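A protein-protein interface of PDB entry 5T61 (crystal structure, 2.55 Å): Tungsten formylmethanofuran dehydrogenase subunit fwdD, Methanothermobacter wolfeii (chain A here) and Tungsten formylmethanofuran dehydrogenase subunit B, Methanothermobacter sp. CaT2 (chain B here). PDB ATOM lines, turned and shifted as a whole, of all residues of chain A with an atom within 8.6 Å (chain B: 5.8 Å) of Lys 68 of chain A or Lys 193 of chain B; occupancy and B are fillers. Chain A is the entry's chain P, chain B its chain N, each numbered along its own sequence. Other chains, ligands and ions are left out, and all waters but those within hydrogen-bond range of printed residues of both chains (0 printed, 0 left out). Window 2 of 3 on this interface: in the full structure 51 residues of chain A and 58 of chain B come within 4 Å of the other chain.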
ATOM      1  N   TRP A  12      -0.896  -8.503  16.335  1.00  0.00           N
ATOM      2  CA  TRP A  12      -1.676  -8.157  15.154  1.00  0.00           C
ATOM      3  C   TRP A  12      -3.155  -8.468  15.340  1.00  0.00           C
ATOM      4  O   TRP A  12      -4.015  -7.729  14.846  1.00  0.00           O
ATOM      5  CB  TRP A  12      -1.103  -8.879  13.936  1.00  0.00           C
ATOM      6  CG  TRP A  12       0.376  -8.747  13.920  1.00  0.00           C
ATOM      7  CD1 TRP A  12       1.294  -9.744  14.053  1.00  0.00           C
ATOM      8  CD2 TRP A  12       1.116  -7.524  13.843  1.00  0.00           C
ATOM      9  NE1 TRP A  12       2.564  -9.220  14.030  1.00  0.00           N
ATOM     10  CE2 TRP A  12       2.482  -7.858  13.901  1.00  0.00           C
ATOM     11  CE3 TRP A  12       0.756  -6.178  13.713  1.00  0.00           C
ATOM     12  CZ2 TRP A  12       3.488  -6.898  13.834  1.00  0.00           C
ATOM     13  CZ3 TRP A  12       1.754  -5.227  13.647  1.00  0.00           C
ATOM     14  CH2 TRP A  12       3.104  -5.590  13.708  1.00  0.00           C
ATOM     15  N   GLN A  34      -0.372 -20.656  12.072  1.00  0.00           N
ATOM     16  CA  GLN A  34       1.076 -20.508  12.108  1.00  0.00           C
ATOM     17  C   GLN A  34       1.731 -21.879  12.165  1.00  0.00           C
ATOM     18  O   GLN A  34       1.325 -22.735  12.959  1.00  0.00           O
ATOM     19  CB  GLN A  34       1.495 -19.659  13.306  1.00  0.00           C
ATOM     20  CG  GLN A  34       0.898 -18.265  13.296  1.00  0.00           C
ATOM     21  CD  GLN A  34       1.440 -17.397  14.407  1.00  0.00           C
ATOM     22  OE1 GLN A  34       2.222 -17.854  15.242  1.00  0.00           O
ATOM     23  NE2 GLN A  34       1.033 -16.134  14.421  1.00  0.00           N
ATOM     24  N   MET A  35       2.741 -22.089  11.325  1.00  0.00           N
ATOM     25  CA  MET A  35       3.418 -23.375  11.249  1.00  0.00           C
ATOM     26  C   MET A  35       4.923 -23.169  11.152  1.00  0.00           C
ATOM     27  O   MET A  35       5.395 -22.150  10.639  1.00  0.00           O
ATOM     28  CB  MET A  35       2.937 -24.197  10.046  1.00  0.00           C
ATOM     29  CG  MET A  35       1.432 -24.381   9.971  1.00  0.00           C
ATOM     30  SD  MET A  35       0.908 -24.913   8.332  1.00  0.00           S
ATOM     31  CE  MET A  35       1.734 -26.501   8.240  1.00  0.00           C
ATOM     32  N   ASN A  36       5.672 -24.140  11.670  1.00  0.00           N
ATOM     33  CA  ASN A  36       7.103 -24.179  11.422  1.00  0.00           C
ATOM     34  C   ASN A  36       7.366 -24.388   9.934  1.00  0.00           C
ATOM     35  O   ASN A  36       6.593 -25.069   9.250  1.00  0.00           O
ATOM     36  CB  ASN A  36       7.770 -25.301  12.217  1.00  0.00           C
ATOM     37  CG  ASN A  36       7.899 -24.979  13.686  1.00  0.00           C
ATOM     38  OD1 ASN A  36       8.154 -23.835  14.065  1.00  0.00           O
ATOM     39  ND2 ASN A  36       7.751 -25.995  14.527  1.00  0.00           N
ATOM     40  N   PRO A  37       8.442 -23.801   9.400  1.00  0.00           N
ATOM     41  CA  PRO A  37       8.744 -24.007   7.970  1.00  0.00           C
ATOM     42  C   PRO A  37       8.935 -25.470   7.582  1.00  0.00           C
ATOM     43  O   PRO A  37       8.569 -25.834   6.457  1.00  0.00           O
ATOM     44  CB  PRO A  37      10.030 -23.195   7.755  1.00  0.00           C
ATOM     45  CG  PRO A  37      10.220 -22.382   8.979  1.00  0.00           C
ATOM     46  CD  PRO A  37       9.506 -23.059  10.092  1.00  0.00           C
ATOM     47  N   GLU A  47       3.482 -20.147   2.239  1.00  0.00           N
ATOM     48  CA  GLU A  47       2.743 -19.066   2.879  1.00  0.00           C
ATOM     49  C   GLU A  47       1.680 -18.531   1.929  1.00  0.00           C
ATOM     50  O   GLU A  47       1.931 -18.333   0.738  1.00  0.00           O
ATOM     51  CB  GLU A  47       3.679 -17.927   3.290  1.00  0.00           C
ATOM     52  CG  GLU A  47       4.311 -18.044   4.668  1.00  0.00           C
ATOM     53  CD  GLU A  47       4.436 -16.692   5.349  1.00  0.00           C
ATOM     54  OE1 GLU A  47       5.576 -16.237   5.580  1.00  0.00           O
ATOM     55  OE2 GLU A  47       3.389 -16.065   5.618  1.00  0.00           O
ATOM     56  N   VAL A  65       0.608 -19.629   7.574  1.00  0.00           N
ATOM     57  CA  VAL A  65       1.573 -18.573   7.843  1.00  0.00           C
ATOM     58  C   VAL A  65       2.782 -19.215   8.515  1.00  0.00           C
ATOM     59  O   VAL A  65       2.632 -20.130   9.328  1.00  0.00           O
ATOM     60  CB  VAL A  65       0.952 -17.473   8.733  1.00  0.00           C
ATOM     61  CG1 VAL A  65       2.012 -16.757   9.571  1.00  0.00           C
ATOM     62  CG2 VAL A  65       0.135 -16.475   7.892  1.00  0.00           C
ATOM     63  N   GLU A  66       3.982 -18.752   8.164  1.00  0.00           N
ATOM     64  CA  GLU A  66       5.194 -19.273   8.781  1.00  0.00           C
ATOM     65  C   GLU A  66       5.402 -18.609  10.136  1.00  0.00           C
ATOM     66  O   GLU A  66       5.442 -17.379  10.234  1.00  0.00           O
ATOM     67  CB  GLU A  66       6.415 -19.038   7.895  1.00  0.00           C
ATOM     68  CG  GLU A  66       7.679 -19.603   8.519  1.00  0.00           C
ATOM     69  CD  GLU A  66       8.878 -19.584   7.592  1.00  0.00           C
ATOM     70  OE1 GLU A  66       8.839 -20.237   6.526  1.00  0.00           O
ATOM     71  OE2 GLU A  66       9.879 -18.932   7.958  1.00  0.00           O
ATOM     72  N   ALA A  67       5.542 -19.423  11.180  1.00  0.00           N
ATOM     73  CA  ALA A  67       5.673 -18.919  12.545  1.00  0.00           C
ATOM     74  C   ALA A  67       6.993 -18.180  12.756  1.00  0.00           C
ATOM     75  O   ALA A  67       8.074 -18.737  12.536  1.00  0.00           O
ATOM     76  CB  ALA A  67       5.548 -20.071  13.535  1.00  0.00           C
ATOM     77  N   LYS A  68       6.896 -16.924  13.198  1.00  0.00           N
ATOM     78  CA  LYS A  68       8.058 -16.166  13.646  1.00  0.00           C
ATOM     79  C   LYS A  68       8.394 -16.435  15.109  1.00  0.00           C
ATOM     80  O   LYS A  68       9.514 -16.142  15.545  1.00  0.00           O
ATOM     81  CB  LYS A  68       7.801 -14.671  13.469  1.00  0.00           C
ATOM     82  CG  LYS A  68       7.339 -14.200  12.082  1.00  0.00           C
ATOM     83  CD  LYS A  68       7.108 -12.679  12.138  1.00  0.00           C
ATOM     84  CE  LYS A  68       6.948 -11.999  10.771  1.00  0.00           C
ATOM     85  NZ  LYS A  68       8.219 -11.959   9.985  1.00  0.00           N
ATOM     86  N   GLU A  69       7.451 -16.992  15.866  1.00  0.00           N
ATOM     87  CA  GLU A  69       7.678 -17.502  17.206  1.00  0.00           C
ATOM     88  C   GLU A  69       7.735 -19.016  17.100  1.00  0.00           C
ATOM     89  O   GLU A  69       6.683 -19.658  16.952  1.00  0.00           O
ATOM     90  CB  GLU A  69       6.558 -17.063  18.151  1.00  0.00           C
ATOM     91  CG  GLU A  69       6.505 -15.561  18.401  1.00  0.00           C
ATOM     92  CD  GLU A  69       5.267 -15.142  19.173  1.00  0.00           C
ATOM     93  OE1 GLU A  69       5.407 -14.513  20.243  1.00  0.00           O
ATOM     94  OE2 GLU A  69       4.149 -15.448  18.707  1.00  0.00           O
ATOM     95  N   PRO A  70       8.918 -19.631  17.143  1.00  0.00           N
ATOM     96  CA  PRO A  70       9.015 -21.057  16.805  1.00  0.00           C
ATOM     97  C   PRO A  70       8.133 -21.913  17.700  1.00  0.00           C
ATOM     98  O   PRO A  70       7.960 -21.634  18.889  1.00  0.00           O
ATOM     99  CB  PRO A  70      10.501 -21.377  17.009  1.00  0.00           C
ATOM    100  CG  PRO A  70      11.203 -20.074  16.943  1.00  0.00           C
ATOM    101  CD  PRO A  70      10.233 -18.999  17.337  1.00  0.00           C
ATOM    102  N   LEU A  71       7.555 -22.953  17.103  1.00  0.00           N
ATOM    103  CA  LEU A  71       6.685 -23.891  17.782  1.00  0.00           C
ATOM    104  C   LEU A  71       7.437 -25.185  18.064  1.00  0.00           C
ATOM    105  O   LEU A  71       8.377 -25.532  17.341  1.00  0.00           O
ATOM    106  CB  LEU A  71       5.454 -24.202  16.922  1.00  0.00           C
ATOM    107  CG  LEU A  71       4.415 -23.105  16.690  1.00  0.00           C
ATOM    108  CD1 LEU A  71       4.002 -23.072  15.226  1.00  0.00           C
ATOM    109  CD2 LEU A  71       3.204 -23.330  17.578  1.00  0.00           C
ATOM    110  N   LYS B 188       8.829 -20.844  21.730  1.00  0.00           N
ATOM    111  CA  LYS B 188       9.792 -19.756  21.872  1.00  0.00           C
ATOM    112  C   LYS B 188       9.090 -18.480  21.421  1.00  0.00           C
ATOM    113  O   LYS B 188       9.193 -18.034  20.275  1.00  0.00           O
ATOM    114  CB  LYS B 188      11.061 -20.025  21.075  1.00  0.00           C
ATOM    115  CG  LYS B 188      11.523 -21.468  21.123  1.00  0.00           C
ATOM    116  CD  LYS B 188      12.951 -21.600  20.628  1.00  0.00           C
ATOM    117  CE  LYS B 188      13.233 -23.012  20.157  1.00  0.00           C
ATOM    118  NZ  LYS B 188      12.253 -23.432  19.120  1.00  0.00           N
ATOM    119  N   THR B 189       8.327 -17.907  22.347  1.00  0.00           N
ATOM    120  CA  THR B 189       7.640 -16.653  22.107  1.00  0.00           C
ATOM    121  C   THR B 189       8.634 -15.496  22.127  1.00  0.00           C
ATOM    122  O   THR B 189       9.791 -15.635  22.538  1.00  0.00           O
ATOM    123  CB  THR B 189       6.549 -16.430  23.155  1.00  0.00           C
ATOM    124  OG1 THR B 189       7.146 -16.292  24.452  1.00  0.00           O
ATOM    125  CG2 THR B 189       5.582 -17.602  23.173  1.00  0.00           C
ATOM    126  N   ASP B 190       8.175 -14.338  21.648  1.00  0.00           N
ATOM    127  CA  ASP B 190       9.008 -13.143  21.701  1.00  0.00           C
ATOM    128  C   ASP B 190       9.291 -12.722  23.136  1.00  0.00           C
ATOM    129  O   ASP B 190      10.303 -12.067  23.404  1.00  0.00           O
ATOM    130  CB  ASP B 190       8.346 -12.014  20.917  1.00  0.00           C
ATOM    131  CG  ASP B 190       8.316 -12.288  19.428  1.00  0.00           C
ATOM    132  OD1 ASP B 190       9.360 -12.712  18.883  1.00  0.00           O
ATOM    133  OD2 ASP B 190       7.248 -12.101  18.807  1.00  0.00           O
ATOM    134  N   SER B 191       8.412 -13.084  24.071  1.00  0.00           N
ATOM    135  CA  SER B 191       8.719 -12.878  25.481  1.00  0.00           C
ATOM    136  C   SER B 191       9.833 -13.812  25.931  1.00  0.00           C
ATOM    137  O   SER B 191      10.751 -13.399  26.649  1.00  0.00           O
ATOM    138  CB  SER B 191       7.467 -13.096  26.328  1.00  0.00           C
ATOM    139  OG  SER B 191       6.397 -12.289  25.872  1.00  0.00           O
ATOM    140  N   ALA B 192       9.766 -15.077  25.509  1.00  0.00           N
ATOM    141  CA  ALA B 192      10.803 -16.044  25.850  1.00  0.00           C
ATOM    142  C   ALA B 192      12.149 -15.672  25.242  1.00  0.00           C
ATOM    143  O   ALA B 192      13.196 -15.998  25.812  1.00  0.00           O
ATOM    144  CB  ALA B 192      10.383 -17.443  25.399  1.00  0.00           C
ATOM    145  N   LYS B 193      12.146 -15.009  24.083  1.00  0.00           N
ATOM    146  CA  LYS B 193      13.407 -14.647  23.442  1.00  0.00           C
ATOM    147  C   LYS B 193      14.237 -13.696  24.297  1.00  0.00           C
ATOM    148  O   LYS B 193      15.464 -13.652  24.157  1.00  0.00           O
ATOM    149  CB  LYS B 193      13.146 -14.041  22.061  1.00  0.00           C
ATOM    150  CG  LYS B 193      12.821 -15.079  20.992  1.00  0.00           C
ATOM    151  CD  LYS B 193      12.327 -14.452  19.696  1.00  0.00           C
ATOM    152  CE  LYS B 193      11.531 -15.465  18.882  1.00  0.00           C
ATOM    153  NZ  LYS B 193      10.902 -14.875  17.670  1.00  0.00           N
ATOM    154  N   LEU B 194      13.599 -12.928  25.174  1.00  0.00           N
ATOM    155  CA  LEU B 194      14.306 -12.007  26.056  1.00  0.00           C
ATOM    156  C   LEU B 194      14.715 -12.632  27.386  1.00  0.00           C
ATOM    157  O   LEU B 194      15.368 -11.962  28.191  1.00  0.00           O
ATOM    158  CB  LEU B 194      13.444 -10.769  26.319  1.00  0.00           C
ATOM    159  CG  LEU B 194      13.071  -9.973  25.068  1.00  0.00           C
ATOM    160  CD1 LEU B 194      12.073  -8.879  25.413  1.00  0.00           C
ATOM    161  CD2 LEU B 194      14.310  -9.405  24.398  1.00  0.00           C
ATOM    162  N   ALA B 195      14.356 -13.886  27.636  1.00  0.00           N
ATOM    163  CA  ALA B 195      14.533 -14.476  28.955  1.00  0.00           C
ATOM    164  C   ALA B 195      15.965 -14.949  29.170  1.00  0.00           C
ATOM    165  O   ALA B 195      16.674 -15.316  28.227  1.00  0.00           O
ATOM    166  CB  ALA B 195      13.568 -15.645  29.147  1.00  0.00           C
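Of the 8 printed residues of chain B, 4 touch a printed residue of chain A.
Printed residues of chain B that touch a printed residue of chain A: Lys 188, Thr 189, Asp 190 and Lys 193.
Hydrophobic or aromatic side chains of chain A within 4 Å of the printed part of chain B: Pro 70.
Along chain A the printed residues that touch a printed residue of chain B span positions 68 to 70.
Among the printed residues, no Asp or Glu carboxylate lies within 4 Å of a Lys or Arg side-chain nitrogen of the other chain.
Lys 188 of chain B touches Glu 69 of chain A (O to CA, 3.5 Å).
OE1 of Glu 69 of chain A touches CA of Thr 189 of chain B, at 3.6 Å.
N of Lys 188 of chain B sits at hydrogen-bond distance from O of Pro 70 of chain A (3.1 Å).
N of Asp 190 of chain B sits at hydrogen-bond distance from OE1 of Glu 69 of chain A (3.1 Å).
The backbone carbonyl oxygen (O) of Lys 68 of chain A lies within hydrogen-bond range of the side-chain amino group (NZ) of Lys 193 of chain B (2.8 Å).
Of chain B, only Lys 193 comes within 4 Å of Lys 68 of chain A.
Lys 193 of chain B touches just one residue of chain A: Lys 68 (2.8 Å).
No residue of chain A comes within 4 Å of Ala 192 of chain B.
Printed residues of chain A within 4 Å of Asp 190 of chain B: Glu 69 (3.1 Å).
Of the printed residues of chain A, Thr 189 of chain B touches Glu 69 (3.6 Å).
Of the printed residues of chain B, Glu 69 of chain A touches Lys 188, Thr 189 and Asp 190.
Of the printed residues of chain A, Lys 188 of chain B touches Glu 69 and Pro 70.
Of the printed residues of chain B, Pro 70 of chain A touches Lys 188 (3.1 Å).
Pro 37 of chain A touches none of the printed residues of chain B.
The nearest residue of chain B that does not touch Lys 68 of chain A is Asp 190 of chain B (4.8 Å).
The nearest printed residue of chain A that does not touch Lys 188 of chain B is Leu 71 of chain A (4.8 Å).
N of Ser 191 of chain B lies close to OG1 of Thr 189 of chain B (3.5 Å).
The side-chain hydroxyl of Thr 189 of chain B is in hydrogen-bond range of the backbone NH of Ala 192 of chain B (3.1 Å).
NZ of Lys 193 of chain B lies within salt-bridge range of OD1 of Asp 190 of chain B, at 2.9 Å.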
